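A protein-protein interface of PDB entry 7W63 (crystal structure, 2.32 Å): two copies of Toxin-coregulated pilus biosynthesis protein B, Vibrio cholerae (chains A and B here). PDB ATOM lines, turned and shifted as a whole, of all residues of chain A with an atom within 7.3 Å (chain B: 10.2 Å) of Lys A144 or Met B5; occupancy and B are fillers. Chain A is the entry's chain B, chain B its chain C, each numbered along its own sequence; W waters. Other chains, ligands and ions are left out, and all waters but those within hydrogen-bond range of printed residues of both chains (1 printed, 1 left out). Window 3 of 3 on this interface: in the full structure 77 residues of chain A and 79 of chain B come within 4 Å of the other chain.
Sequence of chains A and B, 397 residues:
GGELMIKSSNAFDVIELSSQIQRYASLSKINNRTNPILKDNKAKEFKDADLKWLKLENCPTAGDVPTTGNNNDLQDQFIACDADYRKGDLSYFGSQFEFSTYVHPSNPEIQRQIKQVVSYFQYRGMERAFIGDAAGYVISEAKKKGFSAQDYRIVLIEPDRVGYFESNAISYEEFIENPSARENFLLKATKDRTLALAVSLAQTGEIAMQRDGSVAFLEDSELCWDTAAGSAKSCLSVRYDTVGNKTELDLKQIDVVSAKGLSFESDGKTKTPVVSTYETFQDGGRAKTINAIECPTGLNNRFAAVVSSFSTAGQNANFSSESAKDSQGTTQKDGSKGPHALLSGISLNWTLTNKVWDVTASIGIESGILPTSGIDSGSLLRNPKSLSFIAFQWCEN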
ATOM      1  N   GLU A   3      19.681  -4.971 -10.673  1.00  0.00           N
ATOM      2  CA  GLU A   3      20.587  -6.088 -10.436  1.00  0.00           C
ATOM      3  C   GLU A   3      19.997  -7.405 -10.931  1.00  0.00           C
ATOM      4  O   GLU A   3      18.942  -7.847 -10.468  1.00  0.00           O
ATOM      5  CB  GLU A   3      20.928  -6.216  -8.953  1.00  0.00           C
ATOM      6  CG  GLU A   3      22.110  -7.139  -8.699  1.00  0.00           C
ATOM      7  CD  GLU A   3      23.438  -6.429  -8.900  1.00  0.00           C
ATOM      8  OE1 GLU A   3      23.869  -5.722  -7.956  1.00  0.00           O
ATOM      9  OE2 GLU A   3      24.038  -6.566  -9.998  1.00  0.00           O
ATOM     10  N   LEU A   4      20.693  -8.036 -11.865  1.00  0.00           N
ATOM     11  CA  LEU A   4      20.228  -9.294 -12.417  1.00  0.00           C
ATOM     12  C   LEU A   4      21.092 -10.465 -11.948  1.00  0.00           C
ATOM     13  O   LEU A   4      21.227 -11.462 -12.645  1.00  0.00           O
ATOM     14  CB  LEU A   4      20.201  -9.216 -13.947  1.00  0.00           C
ATOM     15  CG  LEU A   4      19.148  -8.253 -14.507  1.00  0.00           C
ATOM     16  CD1 LEU A   4      19.477  -7.879 -15.949  1.00  0.00           C
ATOM     17  CD2 LEU A   4      17.734  -8.828 -14.390  1.00  0.00           C
ATOM     18  N   MET A   5      21.664 -10.353 -10.756  1.00  0.00           N
ATOM     19  CA  MET A   5      22.485 -11.438 -10.227  1.00  0.00           C
ATOM     20  C   MET A   5      21.824 -12.036  -8.995  1.00  0.00           C
ATOM     21  O   MET A   5      21.394 -11.312  -8.108  1.00  0.00           O
ATOM     22  CB  MET A   5      23.900 -10.935  -9.912  1.00  0.00           C
ATOM     23  CG  MET A   5      24.763 -10.711 -11.166  1.00  0.00           C
ATOM     24  SD  MET A   5      26.372  -9.935 -10.852  1.00  0.00           S
ATOM     25  CE  MET A   5      26.401  -9.950  -9.054  1.00  0.00           C
ATOM     26  N   ILE A   6      21.721 -13.360  -8.948  1.00  0.00           N
ATOM     27  CA  ILE A   6      21.057 -14.016  -7.822  1.00  0.00           C
ATOM     28  C   ILE A   6      22.035 -14.212  -6.673  1.00  0.00           C
ATOM     29  O   ILE A   6      22.944 -15.053  -6.753  1.00  0.00           O
ATOM     30  CB  ILE A   6      20.435 -15.366  -8.229  1.00  0.00           C
ATOM     31  CG1 ILE A   6      19.358 -15.159  -9.293  1.00  0.00           C
ATOM     32  CG2 ILE A   6      19.849 -16.065  -7.007  1.00  0.00           C
ATOM     33  CD1 ILE A   6      18.988 -16.413 -10.047  1.00  0.00           C
ATOM     34  N   LYS A   7      21.849 -13.432  -5.609  1.00  0.00           N
ATOM     35  CA  LYS A   7      22.670 -13.537  -4.417  1.00  0.00           C
ATOM     36  C   LYS A   7      22.538 -14.944  -3.788  1.00  0.00           C
ATOM     37  O   LYS A   7      23.519 -15.684  -3.655  1.00  0.00           O
ATOM     38  CB  LYS A   7      22.312 -12.485  -3.391  1.00  0.00           C
ATOM     39  CG  LYS A   7      23.237 -12.457  -2.184  1.00  0.00           C
ATOM     40  CD  LYS A   7      22.985 -11.244  -1.296  1.00  0.00           C
ATOM     41  CE  LYS A   7      24.257 -10.832  -0.573  1.00  0.00           C
ATOM     42  NZ  LYS A   7      24.060 -10.558   0.885  1.00  0.00           N
ATOM     43  N   ILE A  15      10.864 -17.439  -3.124  1.00  0.00           N
ATOM     44  CA  ILE A  15      10.021 -16.406  -3.706  1.00  0.00           C
ATOM     45  C   ILE A  15       9.319 -16.925  -4.976  1.00  0.00           C
ATOM     46  O   ILE A  15       8.122 -16.728  -5.162  1.00  0.00           O
ATOM     47  CB  ILE A  15      10.862 -15.135  -4.000  1.00  0.00           C
ATOM     48  CG1 ILE A  15      11.461 -14.587  -2.696  1.00  0.00           C
ATOM     49  CG2 ILE A  15      10.033 -14.103  -4.720  1.00  0.00           C
ATOM     50  CD1 ILE A  15      10.492 -14.571  -1.518  1.00  0.00           C
ATOM     51  N   VAL A 138      15.481 -13.667   2.190  1.00  0.00           N
ATOM     52  CA  VAL A 138      14.205 -13.972   1.556  1.00  0.00           C
ATOM     53  C   VAL A 138      13.395 -12.694   1.419  1.00  0.00           C
ATOM     54  O   VAL A 138      12.849 -12.406   0.351  1.00  0.00           O
ATOM     55  CB  VAL A 138      13.416 -15.054   2.334  1.00  0.00           C
ATOM     56  CG1 VAL A 138      11.967 -15.095   1.867  1.00  0.00           C
ATOM     57  CG2 VAL A 138      14.058 -16.402   2.125  1.00  0.00           C
ATOM     58  N   ILE A 139      13.340 -11.915   2.498  1.00  0.00           N
ATOM     59  CA  ILE A 139      12.604 -10.650   2.482  1.00  0.00           C
ATOM     60  C   ILE A 139      13.196  -9.697   1.417  1.00  0.00           C
ATOM     61  O   ILE A 139      12.457  -9.091   0.653  1.00  0.00           O
ATOM     62  CB  ILE A 139      12.579 -10.006   3.894  1.00  0.00           C
ATOM     63  CG1 ILE A 139      11.723 -10.857   4.840  1.00  0.00           C
ATOM     64  CG2 ILE A 139      12.051  -8.566   3.832  1.00  0.00           C
ATOM     65  CD1 ILE A 139      11.843 -10.488   6.324  1.00  0.00           C
ATOM     66  N   SER A 140      14.523  -9.622   1.341  1.00  0.00           N
ATOM     67  CA  SER A 140      15.211  -8.786   0.349  1.00  0.00           C
ATOM     68  C   SER A 140      14.879  -9.198  -1.073  1.00  0.00           C
ATOM     69  O   SER A 140      14.649  -8.350  -1.946  1.00  0.00           O
ATOM     70  CB  SER A 140      16.729  -8.868   0.530  1.00  0.00           C
ATOM     71  OG  SER A 140      17.141  -7.948   1.505  1.00  0.00           O
ATOM     72  N   GLU A 141      14.928 -10.509  -1.297  1.00  0.00           N
ATOM     73  CA  GLU A 141      14.649 -11.100  -2.591  1.00  0.00           C
ATOM     74  C   GLU A 141      13.175 -10.890  -2.985  1.00  0.00           C
ATOM     75  O   GLU A 141      12.885 -10.710  -4.160  1.00  0.00           O
ATOM     76  CB  GLU A 141      15.007 -12.599  -2.577  1.00  0.00           C
ATOM     77  CG  GLU A 141      15.169 -13.247  -3.961  1.00  0.00           C
ATOM     78  CD  GLU A 141      16.344 -12.701  -4.752  1.00  0.00           C
ATOM     79  OE1 GLU A 141      17.369 -12.343  -4.144  1.00  0.00           O
ATOM     80  OE2 GLU A 141      16.257 -12.641  -5.995  1.00  0.00           O
ATOM     81  N   ALA A 142      12.262 -10.906  -2.010  1.00  0.00           N
ATOM     82  CA  ALA A 142      10.831 -10.623  -2.261  1.00  0.00           C
ATOM     83  C   ALA A 142      10.659  -9.257  -2.917  1.00  0.00           C
ATOM     84  O   ALA A 142      10.025  -9.123  -3.972  1.00  0.00           O
ATOM     85  CB  ALA A 142      10.020 -10.687  -0.965  1.00  0.00           C
ATOM     86  N   LYS A 143      11.266  -8.255  -2.296  1.00  0.00           N
ATOM     87  CA  LYS A 143      11.197  -6.894  -2.792  1.00  0.00           C
ATOM     88  C   LYS A 143      11.891  -6.756  -4.138  1.00  0.00           C
ATOM     89  O   LYS A 143      11.410  -6.038  -5.016  1.00  0.00           O
ATOM     90  CB  LYS A 143      11.791  -5.935  -1.762  1.00  0.00           C
ATOM     91  CG  LYS A 143      10.992  -5.944  -0.453  1.00  0.00           C
ATOM     92  CD  LYS A 143      11.564  -4.997   0.602  1.00  0.00           C
ATOM     93  CE  LYS A 143      10.807  -5.139   1.903  1.00  0.00           C
ATOM     94  NZ  LYS A 143      11.493  -4.429   3.018  1.00  0.00           N
ATOM     95  N   LYS A 144      13.001  -7.462  -4.319  1.00  0.00           N
ATOM     96  CA  LYS A 144      13.704  -7.429  -5.603  1.00  0.00           C
ATOM     97  C   LYS A 144      12.832  -7.995  -6.746  1.00  0.00           C
ATOM     98  O   LYS A 144      12.853  -7.494  -7.872  1.00  0.00           O
ATOM     99  CB  LYS A 144      15.014  -8.210  -5.498  1.00  0.00           C
ATOM    100  CG  LYS A 144      15.938  -8.083  -6.690  1.00  0.00           C
ATOM    101  CD  LYS A 144      17.288  -8.701  -6.366  1.00  0.00           C
ATOM    102  CE  LYS A 144      18.214  -8.690  -7.569  1.00  0.00           C
ATOM    103  NZ  LYS A 144      19.577  -9.166  -7.223  1.00  0.00           N
ATOM    104  N   LYS A 145      12.064  -9.031  -6.443  1.00  0.00           N
ATOM    105  CA  LYS A 145      11.255  -9.706  -7.450  1.00  0.00           C
ATOM    106  C   LYS A 145       9.810  -9.191  -7.446  1.00  0.00           C
ATOM    107  O   LYS A 145       8.959  -9.695  -8.181  1.00  0.00           O
ATOM    108  CB  LYS A 145      11.296 -11.232  -7.235  1.00  0.00           C
ATOM    109  CG  LYS A 145      12.705 -11.830  -7.355  1.00  0.00           C
ATOM    110  CD  LYS A 145      12.692 -13.355  -7.226  1.00  0.00           C
ATOM    111  CE  LYS A 145      12.132 -13.996  -8.493  1.00  0.00           C
ATOM    112  NZ  LYS A 145      12.025 -15.478  -8.402  1.00  0.00           N
ATOM    113  N   GLY A 146       9.544  -8.173  -6.630  1.00  0.00           N
ATOM    114  CA  GLY A 146       8.234  -7.550  -6.592  1.00  0.00           C
ATOM    115  C   GLY A 146       7.187  -8.456  -5.979  1.00  0.00           C
ATOM    116  O   GLY A 146       5.997  -8.372  -6.284  1.00  0.00           O
ATOM    117  N   PHE A 147       7.629  -9.350  -5.104  1.00  0.00           N
ATOM    118  CA  PHE A 147       6.678 -10.216  -4.427  1.00  0.00           C
ATOM    119  C   PHE A 147       6.209  -9.552  -3.142  1.00  0.00           C
ATOM    120  O   PHE A 147       7.013  -9.105  -2.326  1.00  0.00           O
ATOM    121  CB  PHE A 147       7.289 -11.579  -4.140  1.00  0.00           C
ATOM    122  CG  PHE A 147       6.418 -12.464  -3.297  1.00  0.00           C
ATOM    123  CD1 PHE A 147       5.271 -13.043  -3.835  1.00  0.00           C
ATOM    124  CD2 PHE A 147       6.740 -12.714  -1.961  1.00  0.00           C
ATOM    125  CE1 PHE A 147       4.458 -13.868  -3.068  1.00  0.00           C
ATOM    126  CE2 PHE A 147       5.939 -13.542  -1.185  1.00  0.00           C
ATOM    127  CZ  PHE A 147       4.784 -14.120  -1.739  1.00  0.00           C
ATOM    128  N   GLU B   3      25.089  -3.049   0.854  1.00  0.00           N
ATOM    129  CA  GLU B   3      24.694  -2.847  -0.529  1.00  0.00           C
ATOM    130  C   GLU B   3      23.722  -1.662  -0.664  1.00  0.00           C
ATOM    131  O   GLU B   3      22.889  -1.417   0.229  1.00  0.00           O
ATOM    132  CB  GLU B   3      24.081  -4.155  -1.094  1.00  0.00           C
ATOM    133  CG  GLU B   3      23.299  -4.046  -2.420  1.00  0.00           C
ATOM    134  CD  GLU B   3      24.099  -3.486  -3.609  1.00  0.00           C
ATOM    135  OE1 GLU B   3      25.300  -3.162  -3.462  1.00  0.00           O
ATOM    136  OE2 GLU B   3      23.505  -3.372  -4.708  1.00  0.00           O
ATOM    137  N   LEU B   4      23.826  -0.939  -1.785  1.00  0.00           N
ATOM    138  CA  LEU B   4      23.032   0.278  -2.003  1.00  0.00           C
ATOM    139  C   LEU B   4      21.726   0.008  -2.770  1.00  0.00           C
ATOM    140  O   LEU B   4      21.121   0.933  -3.333  1.00  0.00           O
ATOM    141  CB  LEU B   4      23.864   1.339  -2.743  1.00  0.00           C
ATOM    142  CG  LEU B   4      24.219   2.596  -1.929  1.00  0.00           C
ATOM    143  CD1 LEU B   4      25.058   3.575  -2.753  1.00  0.00           C
ATOM    144  CD2 LEU B   4      22.973   3.280  -1.356  1.00  0.00           C
ATOM    145  N   MET B   5      21.303  -1.259  -2.780  1.00  0.00           N
ATOM    146  CA  MET B   5      19.941  -1.650  -3.162  1.00  0.00           C
ATOM    147  C   MET B   5      19.021  -1.531  -1.940  1.00  0.00           C
ATOM    148  O   MET B   5      17.945  -2.133  -1.875  1.00  0.00           O
ATOM    149  CB  MET B   5      19.910  -3.078  -3.715  1.00  0.00           C
ATOM    150  CG  MET B   5      19.221  -3.202  -5.078  1.00  0.00           C
ATOM    151  SD  MET B   5      19.001  -4.908  -5.640  1.00  0.00           S
ATOM    152  CE  MET B   5      17.844  -5.501  -4.399  1.00  0.00           C
ATOM    153  N   ILE B   6      19.494  -0.769  -0.955  1.00  0.00           N
ATOM    154  CA  ILE B   6      18.701  -0.347   0.184  1.00  0.00           C
ATOM    155  C   ILE B   6      17.772   0.764  -0.303  1.00  0.00           C
ATOM    156  O   ILE B   6      16.724   1.038   0.288  1.00  0.00           O
ATOM    157  CB  ILE B   6      19.607   0.115   1.358  1.00  0.00           C
ATOM    158  CG1 ILE B   6      18.771   0.418   2.604  1.00  0.00           C
ATOM    159  CG2 ILE B   6      20.457   1.314   0.955  1.00  0.00           C
ATOM    160  CD1 ILE B   6      17.756  -0.661   2.923  1.00  0.00           C
ATOM    161  N   LYS B   7      18.157   1.388  -1.409  1.00  0.00           N
ATOM    162  CA  LYS B   7      17.340   2.435  -1.988  1.00  0.00           C
ATOM    163  C   LYS B   7      16.095   1.857  -2.664  1.00  0.00           C
ATOM    164  O   LYS B   7      14.989   2.355  -2.448  1.00  0.00           O
ATOM    165  CB  LYS B   7      18.165   3.270  -2.967  1.00  0.00           C
ATOM    166  CG  LYS B   7      18.673   4.551  -2.321  1.00  0.00           C
ATOM    167  CD  LYS B   7      19.337   5.497  -3.296  1.00  0.00           C
ATOM    168  CE  LYS B   7      20.815   5.150  -3.470  1.00  0.00           C
ATOM    169  NZ  LYS B   7      21.420   5.709  -4.731  1.00  0.00           N
ATOM    170  N   SER B   8      16.269   0.800  -3.462  1.00  0.00           N
ATOM    171  CA  SER B   8      15.141   0.188  -4.162  1.00  0.00           C
ATOM    172  C   SER B   8      14.177  -0.493  -3.183  1.00  0.00           C
ATOM    173  O   SER B   8      12.965  -0.500  -3.397  1.00  0.00           O
ATOM    174  CB  SER B   8      15.636  -0.811  -5.217  1.00  0.00           C
ATOM    175  OG  SER B   8      16.383  -1.858  -4.628  1.00  0.00           O
ATOM    176  N   SER B   9      14.724  -1.038  -2.098  1.00  0.00           N
ATOM    177  CA  SER B   9      13.943  -1.722  -1.071  1.00  0.00           C
ATOM    178  C   SER B   9      13.136  -0.744  -0.200  1.00  0.00           C
ATOM    179  O   SER B   9      11.999  -1.044   0.226  1.00  0.00           O
ATOM    180  CB  SER B   9      14.880  -2.562  -0.205  1.00  0.00           C
ATOM    181  OG  SER B   9      14.394  -2.705   1.122  1.00  0.00           O
ATOM    182  N   ASN B  10      13.728   0.421   0.065  1.00  0.00           N
ATOM    183  CA  ASN B  10      13.032   1.485   0.778  1.00  0.00           C
ATOM    184  C   ASN B  10      11.883   1.931  -0.109  1.00  0.00           C
ATOM    185  O   ASN B  10      10.740   2.066   0.348  1.00  0.00           O
ATOM    186  CB  ASN B  10      13.986   2.636   1.095  1.00  0.00           C
ATOM    187  CG  ASN B  10      13.336   3.776   1.902  1.00  0.00           C
ATOM    188  OD1 ASN B  10      13.788   4.916   1.822  1.00  0.00           O
ATOM    189  ND2 ASN B  10      12.311   3.469   2.693  1.00  0.00           N
ATOM    190  N   ALA B  11      12.187   2.095  -1.393  1.00  0.00           N
ATOM    191  CA  ALA B  11      11.202   2.537  -2.368  1.00  0.00           C
ATOM    192  C   ALA B  11      10.031   1.558  -2.493  1.00  0.00           C
ATOM    193  O   ALA B  11       8.876   1.978  -2.636  1.00  0.00           O
ATOM    194  CB  ALA B  11      11.863   2.743  -3.721  1.00  0.00           C
ATOM    195  N   PHE B  12      10.332   0.264  -2.446  1.00  0.00           N
ATOM    196  CA  PHE B  12       9.298  -0.769  -2.570  1.00  0.00           C
ATOM    197  C   PHE B  12       8.241  -0.583  -1.478  1.00  0.00           C
ATOM    198  O   PHE B  12       7.041  -0.621  -1.747  1.00  0.00           O
ATOM    199  CB  PHE B  12       9.914  -2.175  -2.491  1.00  0.00           C
ATOM    200  CG  PHE B  12       8.901  -3.294  -2.506  1.00  0.00           C
ATOM    201  CD1 PHE B  12       8.448  -3.828  -3.709  1.00  0.00           C
ATOM    202  CD2 PHE B  12       8.399  -3.810  -1.321  1.00  0.00           C
ATOM    203  CE1 PHE B  12       7.505  -4.859  -3.727  1.00  0.00           C
ATOM    204  CE2 PHE B  12       7.451  -4.844  -1.332  1.00  0.00           C
ATOM    205  CZ  PHE B  12       7.012  -5.369  -2.536  1.00  0.00           C
ATOM    206  N   ASP B  13       8.703  -0.367  -0.252  1.00  0.00           N
ATOM    207  CA  ASP B  13       7.826  -0.118   0.888  1.00  0.00           C
ATOM    208  C   ASP B  13       7.013   1.171   0.726  1.00  0.00           C
ATOM    209  O   ASP B  13       5.840   1.198   1.079  1.00  0.00           O
ATOM    210  CB  ASP B  13       8.640  -0.053   2.184  1.00  0.00           C
ATOM    211  CG  ASP B  13       9.228  -1.404   2.578  1.00  0.00           C
ATOM    212  OD1 ASP B  13       8.555  -2.439   2.363  1.00  0.00           O
ATOM    213  OD2 ASP B  13      10.362  -1.433   3.108  1.00  0.00           O
ATOM    214  N   ASP B  89      15.444   5.902   4.465  1.00  0.00           N
ATOM    215  CA  ASP B  89      15.724   7.274   4.075  1.00  0.00           C
ATOM    216  C   ASP B  89      14.438   8.005   3.739  1.00  0.00           C
ATOM    217  O   ASP B  89      14.312   9.188   4.022  1.00  0.00           O
ATOM    218  CB  ASP B  89      16.691   7.322   2.898  1.00  0.00           C
ATOM    219  CG  ASP B  89      18.122   7.029   3.312  1.00  0.00           C
ATOM    220  OD1 ASP B  89      18.380   6.919   4.533  1.00  0.00           O
ATOM    221  OD2 ASP B  89      18.983   6.930   2.411  1.00  0.00           O
ATOM    222  N   ASP B 133      17.534  11.545  -5.989  1.00  0.00           N
ATOM    223  CA  ASP B 133      17.990  10.183  -6.228  1.00  0.00           C
ATOM    224  C   ASP B 133      17.084   9.141  -5.568  1.00  0.00           C
ATOM    225  O   ASP B 133      16.667   8.182  -6.222  1.00  0.00           O
ATOM    226  CB  ASP B 133      19.420  10.020  -5.729  1.00  0.00           C
ATOM    227  CG  ASP B 133      20.007   8.675  -6.085  1.00  0.00           C
ATOM    228  OD1 ASP B 133      20.168   8.387  -7.295  1.00  0.00           O
ATOM    229  OD2 ASP B 133      20.301   7.901  -5.148  1.00  0.00           O
ATOM    230  N   TYR B 137      14.000   5.997  -7.353  1.00  0.00           N
ATOM    231  CA  TYR B 137      13.720   4.613  -7.026  1.00  0.00           C
ATOM    232  C   TYR B 137      12.240   4.417  -6.726  1.00  0.00           C
ATOM    233  O   TYR B 137      11.662   3.374  -7.066  1.00  0.00           O
ATOM    234  CB  TYR B 137      14.583   4.159  -5.844  1.00  0.00           C
ATOM    235  CG  TYR B 137      16.010   3.936  -6.279  1.00  0.00           C
ATOM    236  CD1 TYR B 137      16.386   2.744  -6.903  1.00  0.00           C
ATOM    237  CD2 TYR B 137      16.972   4.930  -6.117  1.00  0.00           C
ATOM    238  CE1 TYR B 137      17.683   2.542  -7.338  1.00  0.00           C
ATOM    239  CE2 TYR B 137      18.277   4.735  -6.543  1.00  0.00           C
ATOM    240  CZ  TYR B 137      18.627   3.538  -7.151  1.00  0.00           C
ATOM    241  OH  TYR B 137      19.922   3.328  -7.580  1.00  0.00           O
ATOM    242  N   SER B 140      10.394   4.361  -9.938  1.00  0.00           N
ATOM    243  CA  SER B 140      10.661   3.060 -10.539  1.00  0.00           C
ATOM    244  C   SER B 140       9.788   1.957  -9.915  1.00  0.00           C
ATOM    245  O   SER B 140       9.195   1.151 -10.631  1.00  0.00           O
ATOM    246  CB  SER B 140      12.147   2.716 -10.409  1.00  0.00           C
ATOM    247  OG  SER B 140      12.403   1.408 -10.889  1.00  0.00           O
ATOM    248  N   GLU B 141       9.685   1.933  -8.590  1.00  0.00           N
ATOM    249  CA  GLU B 141       8.837   0.950  -7.937  1.00  0.00           C
ATOM    250  C   GLU B 141       7.382   1.165  -8.316  1.00  0.00           C
ATOM    251  O   GLU B 141       6.611   0.204  -8.391  1.00  0.00           O
ATOM    252  CB  GLU B 141       8.998   1.007  -6.421  1.00  0.00           C
ATOM    253  CG  GLU B 141      10.334   0.474  -5.923  1.00  0.00           C
ATOM    254  CD  GLU B 141      10.619  -0.955  -6.396  1.00  0.00           C
ATOM    255  OE1 GLU B 141       9.670  -1.769  -6.448  1.00  0.00           O
ATOM    256  OE2 GLU B 141      11.789  -1.273  -6.696  1.00  0.00           O
ATOM    257  N   LYS B 144       6.490  -0.371 -11.775  1.00  0.00           N
ATOM    258  CA  LYS B 144       6.434  -1.828 -11.664  1.00  0.00           C
ATOM    259  C   LYS B 144       5.076  -2.334 -11.192  1.00  0.00           C
ATOM    260  O   LYS B 144       4.724  -3.494 -11.428  1.00  0.00           O
ATOM    261  CB  LYS B 144       7.496  -2.329 -10.690  1.00  0.00           C
ATOM    262  CG  LYS B 144       8.889  -2.340 -11.225  1.00  0.00           C
ATOM    263  CD  LYS B 144       9.806  -2.980 -10.195  1.00  0.00           C
ATOM    264  CE  LYS B 144      11.243  -2.618 -10.466  1.00  0.00           C
ATOM    265  NZ  LYS B 144      12.128  -3.238  -9.458  1.00  0.00           N
ATOM    266  N   LYS B 145       4.339  -1.474 -10.495  1.00  0.00           N
ATOM    267  CA  LYS B 145       3.060  -1.858  -9.915  1.00  0.00           C
ATOM    268  C   LYS B 145       1.923  -1.222 -10.699  1.00  0.00           C
ATOM    269  O   LYS B 145       0.799  -1.145 -10.218  1.00  0.00           O
ATOM    270  CB  LYS B 145       2.990  -1.441  -8.442  1.00  0.00           C
ATOM    271  CG  LYS B 145       3.878  -2.248  -7.499  1.00  0.00           C
ATOM    272  CD  LYS B 145       3.294  -3.636  -7.224  1.00  0.00           C
ATOM    273  CE  LYS B 145       4.306  -4.523  -6.477  1.00  0.00           C
ATOM    274  NZ  LYS B 145       3.775  -5.884  -6.152  1.00  0.00           N
HETATM  275  O   HOH W   1      10.353  -4.615  -7.226  1.00  0.00           O
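Among the printed residues, merely in contact across the chains: Lys A143 with Phe B12, Lys A143 with Ser B9, Phe A147 with Phe B12, Lys A144 with Met B5 and Gly A146 with Phe B12.
Lys A144 touches one residue of chain B. Printed residues of chain A within 4 Å of Met B5: Lys A144 (3.8 Å). No residue of chain B comes within 4 Å of Glu A3. No residue of chain B comes within 4 Å of Ala A142. Of the printed residues of chain A, Phe B12 touches Lys A143, Gly A146 and Phe A147. Of the printed residues of chain A, Asp B13 touches Lys A143. The nearest residue of chain B that does not touch Lys A144 is Lys B144 (4.6 Å).
Of the 16 printed residues of chain A, 4 touch a printed residue of chain B. Along chain A the printed residues that touch a printed residue of chain B span positions 143 to 147. Hydrophobic or aromatic side chains of chain B that line the printed part of chain A: Met B5 and Phe B12. Among the printed residues, 7 pairs touch across the chains. Among the printed residues, Asp or Glu carboxylates within 4 Å of a Lys or Arg side-chain nitrogen of the other chain: Lys A143 with Asp B13 (3.2 Å).
Lys A144 touches Met B5, but with the chains exchanged Met A5 does not touch Lys B144 (12.0 Å). Positions printed for both chains: 3, 4, 5, 6, 7, 140, 141, 144 and 145.
Water W1 lies within hydrogen-bond range of the backbone carbonyl oxygen (O) of Lys A143 (2.8 Å), the side-chain carboxylate (OE1) of Glu B141 (3.0 Å) and the side-chain amino group (NZ) of Lys B144 (3.2 Å).
The backbone carbonyl oxygen (O) of Ala A142 sits at hydrogen-bond distance from the backbone NH (N) of Phe A147, 2.7 Å away. The side-chain hydroxyl (OG) of Ser B8 lies close to the backbone carbonyl oxygen (O) of Met B5 (3.2 Å). O of Met A5 sits at hydrogen-bond distance from NZ of Lys A144 (2.9 Å).
The side-chain amino group (NZ) of Lys A143 is in salt-bridge range of the side-chain carboxylate (OD2) of Asp B13. O of Gly A146 lies within hydrogen-bond range of NZ of Lys B145 (3.3 Å).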
